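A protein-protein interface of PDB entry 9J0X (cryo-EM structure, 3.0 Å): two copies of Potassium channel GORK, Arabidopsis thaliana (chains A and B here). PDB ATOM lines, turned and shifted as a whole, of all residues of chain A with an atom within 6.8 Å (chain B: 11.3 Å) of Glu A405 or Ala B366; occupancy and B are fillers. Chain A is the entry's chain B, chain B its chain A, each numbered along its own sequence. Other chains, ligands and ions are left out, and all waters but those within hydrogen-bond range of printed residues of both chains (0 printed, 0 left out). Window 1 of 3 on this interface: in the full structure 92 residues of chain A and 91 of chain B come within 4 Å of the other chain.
The guanidinium group (NE) of Arg B369 sits at hydrogen-bond distance from the backbone carbonyl oxygen (O) of Ile B364 (2.7 Å). The backbone carbonyl oxygen of Tyr A406 sits at hydrogen-bond distance from a ring nitrogen (NE2) of His A346 (3.0 Å). The backbone carbonyl oxygen (O) of Glu A405 sits at hydrogen-bond distance from the backbone NH (N) of Leu A477, at 2.9 Å. The guanidinium group (NE) of Arg A479 lies within salt-bridge range of the side-chain carboxylate (OE2) of Glu A405, 2.6 Å away. O of Phe A407 sits at hydrogen-bond distance from N of Cys A475 (3.4 Å). ND1 of His A422 sits close to NH1 of Arg A479, at 3.3 Å.
Glu A405 touches two residues of chain B. Of chain A, only Glu A405, His A422 and Tyr A424 come within 4 Å of Ala B366. Tyr A406 touches none of the printed residues of chain B. Phe A407 touches just one residue of chain B: Pro B365 (3.8 Å). No residue of chain B comes within 4 Å of Cys A475. No residue of chain B comes within 4 Å of Arg A479. Of the printed residues of chain A, Ile B364 touches His A346. Of the printed residues of chain A, Pro B365 touches His A346, Glu A405 and Phe A407. Printed residues of chain B within 4 Å of Tyr A424: Ala B366. Of the printed residues of chain B, His A422 touches Ala B366 (3.5 Å). His A403 touches none of the printed residues of chain B.
Among the printed residues, merely in contact across the chains: His A422 with Ala B366, Glu A405 with Pro B365, His A346 with Pro B365, His A346 with Ile B368, Tyr A424 with Ala B366, Phe A407 with Pro B365 and His A346 with Ile B364.
No position is printed for both chains.
The backbone NH (N) of Ala B366 is in hydrogen-bond range of the side-chain carboxylate (OE2) of Glu A405 (3.4 Å). The side-chain hydroxyl (OG) of Ser B367 sits at hydrogen-bond distance from the backbone carbonyl oxygen (O) of Ile A413 (3.0 Å).
Printed residues of chain B that touch a printed residue of chain A: Ile B364, Pro B365, Ala B366, Ser B367 and Ile B368. Hydrophobic or aromatic side chains of chain B within 4 Å of the printed part of chain A: Ile B364, Pro B365, Ala B366 and Ile B368. Of the 16 printed residues of chain A, 6 touch a printed residue of chain B. Printed residues of chain A that touch a printed residue of chain B: His A346, Glu A405, Phe A407, Ile A413, His A422 and Tyr A424. Among the printed residues, 9 pairs touch across the chains.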
ATOM      1  N   HIS A 346      29.870   5.868  19.581  1.00  0.00           N
ATOM      2  CA  HIS A 346      28.427   5.886  19.810  1.00  0.00           C
ATOM      3  C   HIS A 346      27.953   7.215  20.388  1.00  0.00           C
ATOM      4  O   HIS A 346      26.828   7.644  20.097  1.00  0.00           O
ATOM      5  CB  HIS A 346      28.022   4.726  20.716  1.00  0.00           C
ATOM      6  CG  HIS A 346      27.782   3.451  19.975  1.00  0.00           C
ATOM      7  ND1 HIS A 346      28.806   2.681  19.469  1.00  0.00           N
ATOM      8  CD2 HIS A 346      26.635   2.823  19.632  1.00  0.00           C
ATOM      9  CE1 HIS A 346      28.300   1.627  18.856  1.00  0.00           C
ATOM     10  NE2 HIS A 346      26.984   1.687  18.944  1.00  0.00           N
ATOM     11  N   THR A 356      18.383  10.498  18.513  1.00  0.00           N
ATOM     12  CA  THR A 356      17.529   9.557  19.230  1.00  0.00           C
ATOM     13  C   THR A 356      17.094  10.199  20.541  1.00  0.00           C
ATOM     14  O   THR A 356      17.892  10.326  21.476  1.00  0.00           O
ATOM     15  CB  THR A 356      18.273   8.248  19.470  1.00  0.00           C
ATOM     16  OG1 THR A 356      18.702   7.708  18.215  1.00  0.00           O
ATOM     17  CG2 THR A 356      17.365   7.241  20.152  1.00  0.00           C
ATOM     18  N   HIS A 403      13.386  -1.548  21.287  1.00  0.00           N
ATOM     19  CA  HIS A 403      14.285  -0.425  21.501  1.00  0.00           C
ATOM     20  C   HIS A 403      15.090  -0.181  20.234  1.00  0.00           C
ATOM     21  O   HIS A 403      15.561  -1.131  19.604  1.00  0.00           O
ATOM     22  CB  HIS A 403      15.242  -0.682  22.672  1.00  0.00           C
ATOM     23  CG  HIS A 403      14.555  -0.859  23.988  1.00  0.00           C
ATOM     24  ND1 HIS A 403      14.311   0.191  24.847  1.00  0.00           N
ATOM     25  CD2 HIS A 403      14.070  -1.964  24.599  1.00  0.00           C
ATOM     26  CE1 HIS A 403      13.700  -0.259  25.927  1.00  0.00           C
ATOM     27  NE2 HIS A 403      13.542  -1.564  25.803  1.00  0.00           N
ATOM     28  N   GLU A 404      15.257   1.087  19.871  1.00  0.00           N
ATOM     29  CA  GLU A 404      16.058   1.456  18.712  1.00  0.00           C
ATOM     30  C   GLU A 404      17.520   1.598  19.108  1.00  0.00           C
ATOM     31  O   GLU A 404      17.841   2.194  20.139  1.00  0.00           O
ATOM     32  CB  GLU A 404      15.569   2.767  18.096  1.00  0.00           C
ATOM     33  CG  GLU A 404      14.224   2.689  17.408  1.00  0.00           C
ATOM     34  CD  GLU A 404      13.813   4.015  16.802  1.00  0.00           C
ATOM     35  OE1 GLU A 404      14.508   5.023  17.049  1.00  0.00           O
ATOM     36  OE2 GLU A 404      12.803   4.052  16.068  1.00  0.00           O
ATOM     37  N   GLU A 405      18.406   1.049  18.280  1.00  0.00           N
ATOM     38  CA  GLU A 405      19.840   1.106  18.520  1.00  0.00           C
ATOM     39  C   GLU A 405      20.569   1.305  17.202  1.00  0.00           C
ATOM     40  O   GLU A 405      20.169   0.753  16.174  1.00  0.00           O
ATOM     41  CB  GLU A 405      20.340  -0.166  19.215  1.00  0.00           C
ATOM     42  CG  GLU A 405      20.068  -0.190  20.710  1.00  0.00           C
ATOM     43  CD  GLU A 405      20.411  -1.512  21.351  1.00  0.00           C
ATOM     44  OE1 GLU A 405      20.778  -2.456  20.622  1.00  0.00           O
ATOM     45  OE2 GLU A 405      20.327  -1.598  22.593  1.00  0.00           O
ATOM     46  N   TYR A 406      21.639   2.094  17.240  1.00  0.00           N
ATOM     47  CA  TYR A 406      22.438   2.418  16.066  1.00  0.00           C
ATOM     48  C   TYR A 406      23.873   1.973  16.296  1.00  0.00           C
ATOM     49  O   TYR A 406      24.426   2.176  17.381  1.00  0.00           O
ATOM     50  CB  TYR A 406      22.417   3.920  15.773  1.00  0.00           C
ATOM     51  CG  TYR A 406      21.079   4.490  15.367  1.00  0.00           C
ATOM     52  CD1 TYR A 406      20.783   4.725  14.032  1.00  0.00           C
ATOM     53  CD2 TYR A 406      20.125   4.825  16.321  1.00  0.00           C
ATOM     54  CE1 TYR A 406      19.565   5.256  13.655  1.00  0.00           C
ATOM     55  CE2 TYR A 406      18.906   5.356  15.955  1.00  0.00           C
ATOM     56  CZ  TYR A 406      18.633   5.573  14.623  1.00  0.00           C
ATOM     57  OH  TYR A 406      17.419   6.102  14.255  1.00  0.00           O
ATOM     58  N   PHE A 407      24.484   1.378  15.274  1.00  0.00           N
ATOM     59  CA  PHE A 407      25.845   0.870  15.380  1.00  0.00           C
ATOM     60  C   PHE A 407      26.668   1.334  14.190  1.00  0.00           C
ATOM     61  O   PHE A 407      26.197   1.308  13.052  1.00  0.00           O
ATOM     62  CB  PHE A 407      25.864  -0.661  15.453  1.00  0.00           C
ATOM     63  CG  PHE A 407      25.268  -1.218  16.712  1.00  0.00           C
ATOM     64  CD1 PHE A 407      26.066  -1.481  17.812  1.00  0.00           C
ATOM     65  CD2 PHE A 407      23.914  -1.488  16.791  1.00  0.00           C
ATOM     66  CE1 PHE A 407      25.522  -1.994  18.971  1.00  0.00           C
ATOM     67  CE2 PHE A 407      23.363  -2.001  17.946  1.00  0.00           C
ATOM     68  CZ  PHE A 407      24.168  -2.254  19.037  1.00  0.00           C
ATOM     69  N   ILE A 413      28.321  -7.300  17.360  1.00  0.00           N
ATOM     70  CA  ILE A 413      27.154  -7.230  18.230  1.00  0.00           C
ATOM     71  C   ILE A 413      27.024  -8.532  19.005  1.00  0.00           C
ATOM     72  O   ILE A 413      27.139  -8.553  20.235  1.00  0.00           O
ATOM     73  CB  ILE A 413      25.891  -6.945  17.409  1.00  0.00           C
ATOM     74  CG1 ILE A 413      26.139  -5.757  16.490  1.00  0.00           C
ATOM     75  CG2 ILE A 413      24.722  -6.666  18.324  1.00  0.00           C
ATOM     76  CD1 ILE A 413      25.207  -5.705  15.340  1.00  0.00           C
ATOM     77  N   HIS A 422      19.825 -10.830  23.601  1.00  0.00           N
ATOM     78  CA  HIS A 422      18.907  -9.920  22.934  1.00  0.00           C
ATOM     79  C   HIS A 422      18.592 -10.431  21.539  1.00  0.00           C
ATOM     80  O   HIS A 422      19.453 -11.006  20.870  1.00  0.00           O
ATOM     81  CB  HIS A 422      19.483  -8.503  22.838  1.00  0.00           C
ATOM     82  CG  HIS A 422      19.783  -7.880  24.164  1.00  0.00           C
ATOM     83  ND1 HIS A 422      18.825  -7.244  24.922  1.00  0.00           N
ATOM     84  CD2 HIS A 422      20.936  -7.796  24.867  1.00  0.00           C
ATOM     85  CE1 HIS A 422      19.375  -6.793  26.034  1.00  0.00           C
ATOM     86  NE2 HIS A 422      20.656  -7.115  26.026  1.00  0.00           N
ATOM     87  N   TYR A 424      17.464  -9.202  17.781  1.00  0.00           N
ATOM     88  CA  TYR A 424      17.628  -7.990  16.996  1.00  0.00           C
ATOM     89  C   TYR A 424      16.896  -8.106  15.668  1.00  0.00           C
ATOM     90  O   TYR A 424      16.939  -9.153  15.017  1.00  0.00           O
ATOM     91  CB  TYR A 424      19.101  -7.705  16.725  1.00  0.00           C
ATOM     92  CG  TYR A 424      19.899  -7.252  17.923  1.00  0.00           C
ATOM     93  CD1 TYR A 424      19.801  -5.952  18.395  1.00  0.00           C
ATOM     94  CD2 TYR A 424      20.766  -8.122  18.571  1.00  0.00           C
ATOM     95  CE1 TYR A 424      20.534  -5.532  19.486  1.00  0.00           C
ATOM     96  CE2 TYR A 424      21.501  -7.712  19.664  1.00  0.00           C
ATOM     97  CZ  TYR A 424      21.383  -6.416  20.114  1.00  0.00           C
ATOM     98  OH  TYR A 424      22.113  -5.999  21.200  1.00  0.00           O
ATOM     99  N   CYS A 475      23.622   0.953  10.797  1.00  0.00           N
ATOM    100  CA  CYS A 475      22.374   0.221  10.941  1.00  0.00           C
ATOM    101  C   CYS A 475      21.494   0.831  12.025  1.00  0.00           C
ATOM    102  O   CYS A 475      21.913   1.688  12.805  1.00  0.00           O
ATOM    103  CB  CYS A 475      22.648  -1.256  11.241  1.00  0.00           C
ATOM    104  SG  CYS A 475      23.656  -1.556  12.696  1.00  0.00           S
ATOM    105  N   HIS A 476      20.251   0.359  12.053  1.00  0.00           N
ATOM    106  CA  HIS A 476      19.161   0.878  12.876  1.00  0.00           C
ATOM    107  C   HIS A 476      18.409  -0.278  13.531  1.00  0.00           C
ATOM    108  O   HIS A 476      17.206  -0.458  13.342  1.00  0.00           O
ATOM    109  CB  HIS A 476      18.248   1.768  12.033  1.00  0.00           C
ATOM    110  CG  HIS A 476      17.197   2.492  12.817  1.00  0.00           C
ATOM    111  ND1 HIS A 476      16.103   3.081  12.222  1.00  0.00           N
ATOM    112  CD2 HIS A 476      17.054   2.692  14.149  1.00  0.00           C
ATOM    113  CE1 HIS A 476      15.341   3.628  13.152  1.00  0.00           C
ATOM    114  NE2 HIS A 476      15.896   3.407  14.329  1.00  0.00           N
ATOM    115  N   LEU A 477      19.142  -1.132  14.243  1.00  0.00           N
ATOM    116  CA  LEU A 477      18.576  -2.363  14.785  1.00  0.00           C
ATOM    117  C   LEU A 477      17.492  -2.101  15.824  1.00  0.00           C
ATOM    118  O   LEU A 477      17.548  -1.128  16.580  1.00  0.00           O
ATOM    119  CB  LEU A 477      19.671  -3.206  15.425  1.00  0.00           C
ATOM    120  CG  LEU A 477      20.942  -3.469  14.637  1.00  0.00           C
ATOM    121  CD1 LEU A 477      21.751  -4.448  15.426  1.00  0.00           C
ATOM    122  CD2 LEU A 477      20.615  -4.030  13.278  1.00  0.00           C
ATOM    123  N   LEU A 478      16.497  -2.981  15.844  1.00  0.00           N
ATOM    124  CA  LEU A 478      15.451  -2.984  16.854  1.00  0.00           C
ATOM    125  C   LEU A 478      15.711  -4.149  17.799  1.00  0.00           C
ATOM    126  O   LEU A 478      15.717  -5.306  17.369  1.00  0.00           O
ATOM    127  CB  LEU A 478      14.071  -3.110  16.211  1.00  0.00           C
ATOM    128  CG  LEU A 478      13.539  -1.871  15.499  1.00  0.00           C
ATOM    129  CD1 LEU A 478      12.340  -2.225  14.642  1.00  0.00           C
ATOM    130  CD2 LEU A 478      13.176  -0.819  16.517  1.00  0.00           C
ATOM    131  N   ARG A 479      15.916  -3.849  19.075  1.00  0.00           N
ATOM    132  CA  ARG A 479      16.359  -4.840  20.045  1.00  0.00           C
ATOM    133  C   ARG A 479      15.191  -5.318  20.896  1.00  0.00           C
ATOM    134  O   ARG A 479      14.446  -4.505  21.452  1.00  0.00           O
ATOM    135  CB  ARG A 479      17.453  -4.260  20.941  1.00  0.00           C
ATOM    136  CG  ARG A 479      17.892  -5.186  22.052  1.00  0.00           C
ATOM    137  CD  ARG A 479      18.981  -4.563  22.894  1.00  0.00           C
ATOM    138  NE  ARG A 479      18.577  -3.270  23.435  1.00  0.00           N
ATOM    139  CZ  ARG A 479      17.919  -3.114  24.577  1.00  0.00           C
ATOM    140  NH1 ARG A 479      17.586  -4.172  25.301  1.00  0.00           N
ATOM    141  NH2 ARG A 479      17.590  -1.901  24.995  1.00  0.00           N
ATOM    142  N   ASP A 481      14.520  -8.130  24.142  1.00  0.00           N
ATOM    143  CA  ASP A 481      15.240  -8.899  25.147  1.00  0.00           C
ATOM    144  C   ASP A 481      14.927 -10.388  25.031  1.00  0.00           C
ATOM    145  O   ASP A 481      13.970 -10.805  24.373  1.00  0.00           O
ATOM    146  CB  ASP A 481      14.892  -8.408  26.549  1.00  0.00           C
ATOM    147  CG  ASP A 481      15.173  -6.934  26.732  1.00  0.00           C
ATOM    148  OD1 ASP A 481      14.480  -6.113  26.098  1.00  0.00           O
ATOM    149  OD2 ASP A 481      16.086  -6.595  27.514  1.00  0.00           O
ATOM    150  N   THR B 358      25.697   5.570  36.172  1.00  0.00           N
ATOM    151  CA  THR B 358      25.351   4.877  34.939  1.00  0.00           C
ATOM    152  C   THR B 358      24.364   5.684  34.095  1.00  0.00           C
ATOM    153  O   THR B 358      24.126   5.349  32.929  1.00  0.00           O
ATOM    154  CB  THR B 358      24.798   3.486  35.308  1.00  0.00           C
ATOM    155  OG1 THR B 358      25.631   2.914  36.322  1.00  0.00           O
ATOM    156  CG2 THR B 358      24.835   2.507  34.126  1.00  0.00           C
ATOM    157  N   LEU B 361      25.530   6.679  30.845  1.00  0.00           N
ATOM    158  CA  LEU B 361      25.642   5.604  29.873  1.00  0.00           C
ATOM    159  C   LEU B 361      24.301   5.139  29.321  1.00  0.00           C
ATOM    160  O   LEU B 361      24.276   4.217  28.500  1.00  0.00           O
ATOM    161  CB  LEU B 361      26.380   4.413  30.488  1.00  0.00           C
ATOM    162  CG  LEU B 361      27.890   4.529  30.645  1.00  0.00           C
ATOM    163  CD1 LEU B 361      28.404   3.466  31.595  1.00  0.00           C
ATOM    164  CD2 LEU B 361      28.575   4.413  29.297  1.00  0.00           C
ATOM    165  N   GLN B 362      23.183   5.744  29.733  1.00  0.00           N
ATOM    166  CA  GLN B 362      21.884   5.263  29.260  1.00  0.00           C
ATOM    167  C   GLN B 362      21.472   5.831  27.902  1.00  0.00           C
ATOM    168  O   GLN B 362      20.315   6.187  27.679  1.00  0.00           O
ATOM    169  CB  GLN B 362      20.834   5.547  30.335  1.00  0.00           C
ATOM    170  CG  GLN B 362      20.812   6.977  30.882  1.00  0.00           C
ATOM    171  CD  GLN B 362      19.837   7.905  30.182  1.00  0.00           C
ATOM    172  OE1 GLN B 362      18.773   7.483  29.732  1.00  0.00           O
ATOM    173  NE2 GLN B 362      20.201   9.179  30.084  1.00  0.00           N
ATOM    174  N   ASP B 363      22.411   5.862  26.961  1.00  0.00           N
ATOM    175  CA  ASP B 363      22.158   5.870  25.529  1.00  0.00           C
ATOM    176  C   ASP B 363      23.122   4.964  24.786  1.00  0.00           C
ATOM    177  O   ASP B 363      22.889   4.678  23.609  1.00  0.00           O
ATOM    178  CB  ASP B 363      22.246   7.294  24.962  1.00  0.00           C
ATOM    179  CG  ASP B 363      20.995   8.108  25.230  1.00  0.00           C
ATOM    180  OD1 ASP B 363      19.891   7.532  25.179  1.00  0.00           O
ATOM    181  OD2 ASP B 363      21.114   9.319  25.505  1.00  0.00           O
ATOM    182  N   ILE B 364      24.195   4.520  25.428  1.00  0.00           N
ATOM    183  CA  ILE B 364      25.047   3.453  24.897  1.00  0.00           C
ATOM    184  C   ILE B 364      24.242   2.159  24.861  1.00  0.00           C
ATOM    185  O   ILE B 364      23.557   1.837  25.848  1.00  0.00           O
ATOM    186  CB  ILE B 364      26.303   3.307  25.762  1.00  0.00           C
ATOM    187  CG1 ILE B 364      27.019   4.652  25.891  1.00  0.00           C
ATOM    188  CG2 ILE B 364      27.247   2.271  25.193  1.00  0.00           C
ATOM    189  CD1 ILE B 364      27.509   5.215  24.576  1.00  0.00           C
ATOM    190  N   PRO B 365      24.257   1.415  23.758  1.00  0.00           N
ATOM    191  CA  PRO B 365      23.401   0.230  23.648  1.00  0.00           C
ATOM    192  C   PRO B 365      23.844  -0.910  24.552  1.00  0.00           C
ATOM    193  O   PRO B 365      24.970  -0.952  25.051  1.00  0.00           O
ATOM    194  CB  PRO B 365      23.542  -0.165  22.175  1.00  0.00           C
ATOM    195  CG  PRO B 365      23.949   1.074  21.489  1.00  0.00           C
ATOM    196  CD  PRO B 365      24.829   1.789  22.456  1.00  0.00           C
ATOM    197  N   ALA B 366      22.916  -1.838  24.768  1.00  0.00           N
ATOM    198  CA  ALA B 366      23.255  -3.114  25.373  1.00  0.00           C
ATOM    199  C   ALA B 366      24.155  -3.908  24.432  1.00  0.00           C
ATOM    200  O   ALA B 366      24.172  -3.685  23.217  1.00  0.00           O
ATOM    201  CB  ALA B 366      21.994  -3.908  25.703  1.00  0.00           C
ATOM    202  N   SER B 367      24.918  -4.833  25.029  1.00  0.00           N
ATOM    203  CA  SER B 367      26.101  -5.532  24.511  1.00  0.00           C
ATOM    204  C   SER B 367      27.290  -4.598  24.319  1.00  0.00           C
ATOM    205  O   SER B 367      28.299  -5.003  23.732  1.00  0.00           O
ATOM    206  CB  SER B 367      25.843  -6.321  23.217  1.00  0.00           C
ATOM    207  OG  SER B 367      27.050  -6.578  22.523  1.00  0.00           O
ATOM    208  N   ILE B 368      27.184  -3.345  24.769  1.00  0.00           N
ATOM    209  CA  ILE B 368      28.329  -2.491  25.043  1.00  0.00           C
ATOM    210  C   ILE B 368      28.362  -2.069  26.506  1.00  0.00           C
ATOM    211  O   ILE B 368      29.419  -2.102  27.144  1.00  0.00           O
ATOM    212  CB  ILE B 368      28.345  -1.251  24.123  1.00  0.00           C
ATOM    213  CG1 ILE B 368      28.194  -1.661  22.658  1.00  0.00           C
ATOM    214  CG2 ILE B 368      29.639  -0.472  24.303  1.00  0.00           C
ATOM    215  CD1 ILE B 368      28.271  -0.510  21.690  1.00  0.00           C
ATOM    216  N   ARG B 369      27.208  -1.677  27.054  1.00  0.00           N
ATOM    217  CA  ARG B 369      27.080  -1.483  28.495  1.00  0.00           C
ATOM    218  C   ARG B 369      27.288  -2.791  29.242  1.00  0.00           C
ATOM    219  O   ARG B 369      27.845  -2.807  30.347  1.00  0.00           O
ATOM    220  CB  ARG B 369      25.706  -0.904  28.825  1.00  0.00           C
ATOM    221  CG  ARG B 369      25.714   0.556  29.210  1.00  0.00           C
ATOM    222  CD  ARG B 369      24.316   1.024  29.574  1.00  0.00           C
ATOM    223  NE  ARG B 369      23.422   1.011  28.420  1.00  0.00           N
ATOM    224  CZ  ARG B 369      22.349   0.234  28.315  1.00  0.00           C
ATOM    225  NH1 ARG B 369      22.031  -0.592  29.300  1.00  0.00           N
ATOM    226  NH2 ARG B 369      21.593   0.288  27.227  1.00  0.00           N
ATOM    227  N   ALA B 370      26.843  -3.900  28.648  1.00  0.00           N
ATOM    228  CA  ALA B 370      27.070  -5.209  29.247  1.00  0.00           C
ATOM    229  C   ALA B 370      28.546  -5.577  29.224  1.00  0.00           C
ATOM    230  O   ALA B 370      29.045  -6.202  30.164  1.00  0.00           O
ATOM    231  CB  ALA B 370      26.239  -6.267  28.524  1.00  0.00           C
ATOM    232  N   LYS B 371      29.270  -5.175  28.175  1.00  0.00           N
ATOM    233  CA  LYS B 371      30.706  -5.433  28.137  1.00  0.00           C
ATOM    234  C   LYS B 371      31.456  -4.569  29.139  1.00  0.00           C
ATOM    235  O   LYS B 371      32.450  -5.020  29.715  1.00  0.00           O
ATOM    236  CB  LYS B 371      31.254  -5.205  26.732  1.00  0.00           C
ATOM    237  CG  LYS B 371      30.674  -6.132  25.683  1.00  0.00           C
ATOM    238  CD  LYS B 371      30.789  -7.595  26.078  1.00  0.00           C
ATOM    239  CE  LYS B 371      32.181  -8.140  25.816  1.00  0.00           C
ATOM    240  NZ  LYS B 371      32.200  -9.628  25.862  1.00  0.00           N
ATOM    241  N   ILE B 372      30.979  -3.344  29.377  1.00  0.00           N
ATOM    242  CA  ILE B 372      31.547  -2.501  30.428  1.00  0.00           C
ATOM    243  C   ILE B 372      31.325  -3.138  31.794  1.00  0.00           C
ATOM    244  O   ILE B 372      32.249  -3.240  32.611  1.00  0.00           O
ATOM    245  CB  ILE B 372      30.942  -1.087  30.362  1.00  0.00           C
ATOM    246  CG1 ILE B 372      31.424  -0.352  29.115  1.00  0.00           C
ATOM    247  CG2 ILE B 372      31.290  -0.279  31.600  1.00  0.00           C
ATOM    248  CD1 ILE B 372      30.705   0.951  28.884  1.00  0.00           C
ATOM    249  N   ALA B 373      30.100  -3.609  32.046  1.00  0.00           N
ATOM    250  CA  ALA B 373      29.780  -4.201  33.341  1.00  0.00           C
ATOM    251  C   ALA B 373      30.473  -5.543  33.548  1.00  0.00           C
ATOM    252  O   ALA B 373      30.753  -5.919  34.691  1.00  0.00           O
ATOM    253  CB  ALA B 373      28.270  -4.358  33.480  1.00  0.00           C
ATOM    254  N   GLN B 374      30.767  -6.270  32.472  1.00  0.00           N
ATOM    255  CA  GLN B 374      31.536  -7.501  32.591  1.00  0.00           C
ATOM    256  C   GLN B 374      33.037  -7.254  32.620  1.00  0.00           C
ATOM    257  O   GLN B 374      33.792  -8.150  33.011  1.00  0.00           O
ATOM    258  CB  GLN B 374      31.194  -8.450  31.444  1.00  0.00           C
ATOM    259  CG  GLN B 374      29.823  -9.077  31.560  1.00  0.00           C
ATOM    260  CD  GLN B 374      29.236  -9.433  30.214  1.00  0.00           C
ATOM    261  OE1 GLN B 374      29.935  -9.922  29.330  1.00  0.00           O
ATOM    262  NE2 GLN B 374      27.943  -9.183  30.050  1.00  0.00           N
ATOM    263  N   ASN B 396      25.807 -12.485  34.423  1.00  0.00           N
ATOM    264  CA  ASN B 396      25.710 -11.396  33.454  1.00  0.00           C
ATOM    265  C   ASN B 396      24.450 -10.565  33.664  1.00  0.00           C
ATOM    266  O   ASN B 396      24.430  -9.381  33.315  1.00  0.00           O
ATOM    267  CB  ASN B 396      25.748 -11.941  32.027  1.00  0.00           C
ATOM    268  CG  ASN B 396      27.077 -12.574  31.680  1.00  0.00           C
ATOM    269  OD1 ASN B 396      27.158 -13.425  30.797  1.00  0.00           O
ATOM    270  ND2 ASN B 396      28.128 -12.173  32.385  1.00  0.00           N
ATOM    271  N   GLN B 397      23.395 -11.159  34.224  1.00  0.00           N
ATOM    272  CA  GLN B 397      22.236 -10.356  34.605  1.00  0.00           C
ATOM    273  C   GLN B 397      22.460  -9.610  35.916  1.00  0.00           C
ATOM    274  O   GLN B 397      21.839  -8.566  36.141  1.00  0.00           O
ATOM    275  CB  GLN B 397      20.993 -11.237  34.708  1.00  0.00           C
ATOM    276  CG  GLN B 397      20.482 -11.734  33.369  1.00  0.00           C
ATOM    277  CD  GLN B 397      19.973 -10.613  32.489  1.00  0.00           C
ATOM    278  OE1 GLN B 397      19.198  -9.765  32.931  1.00  0.00           O
ATOM    279  NE2 GLN B 397      20.411 -10.599  31.237  1.00  0.00           N
ATOM    280  N   ILE B 400      24.890  -6.053  35.429  1.00  0.00           N
ATOM    281  CA  ILE B 400      24.379  -4.874  34.734  1.00  0.00           C
ATOM    282  C   ILE B 400      23.800  -3.872  35.727  1.00  0.00           C
ATOM    283  O   ILE B 400      24.046  -2.664  35.632  1.00  0.00           O
ATOM    284  CB  ILE B 400      23.338  -5.295  33.681  1.00  0.00           C
ATOM    285  CG1 ILE B 400      23.977  -6.194  32.628  1.00  0.00           C
ATOM    286  CG2 ILE B 400      22.720  -4.085  33.008  1.00  0.00           C
ATOM    287  CD1 ILE B 400      22.976  -6.838  31.699  1.00  0.00           C
ATOM    288  N   ARG B 401      23.059  -4.360  36.721  1.00  0.00           N
ATOM    289  CA  ARG B 401      22.286  -3.514  37.621  1.00  0.00           C
ATOM    290  C   ARG B 401      23.042  -3.149  38.893  1.00  0.00           C
ATOM    291  O   ARG B 401      22.416  -2.933  39.938  1.00  0.00           O
ATOM    292  CB  ARG B 401      20.968  -4.210  37.956  1.00  0.00           C
ATOM    293  CG  ARG B 401      20.291  -4.781  36.724  1.00  0.00           C
ATOM    294  CD  ARG B 401      19.162  -5.726  37.070  1.00  0.00           C
ATOM    295  NE  ARG B 401      18.394  -6.088  35.884  1.00  0.00           N
ATOM    296  CZ  ARG B 401      18.606  -7.185  35.165  1.00  0.00           C
ATOM    297  NH1 ARG B 401      19.565  -8.030  35.512  1.00  0.00           N
ATOM    298  NH2 ARG B 401      17.860  -7.437  34.099  1.00  0.00           N
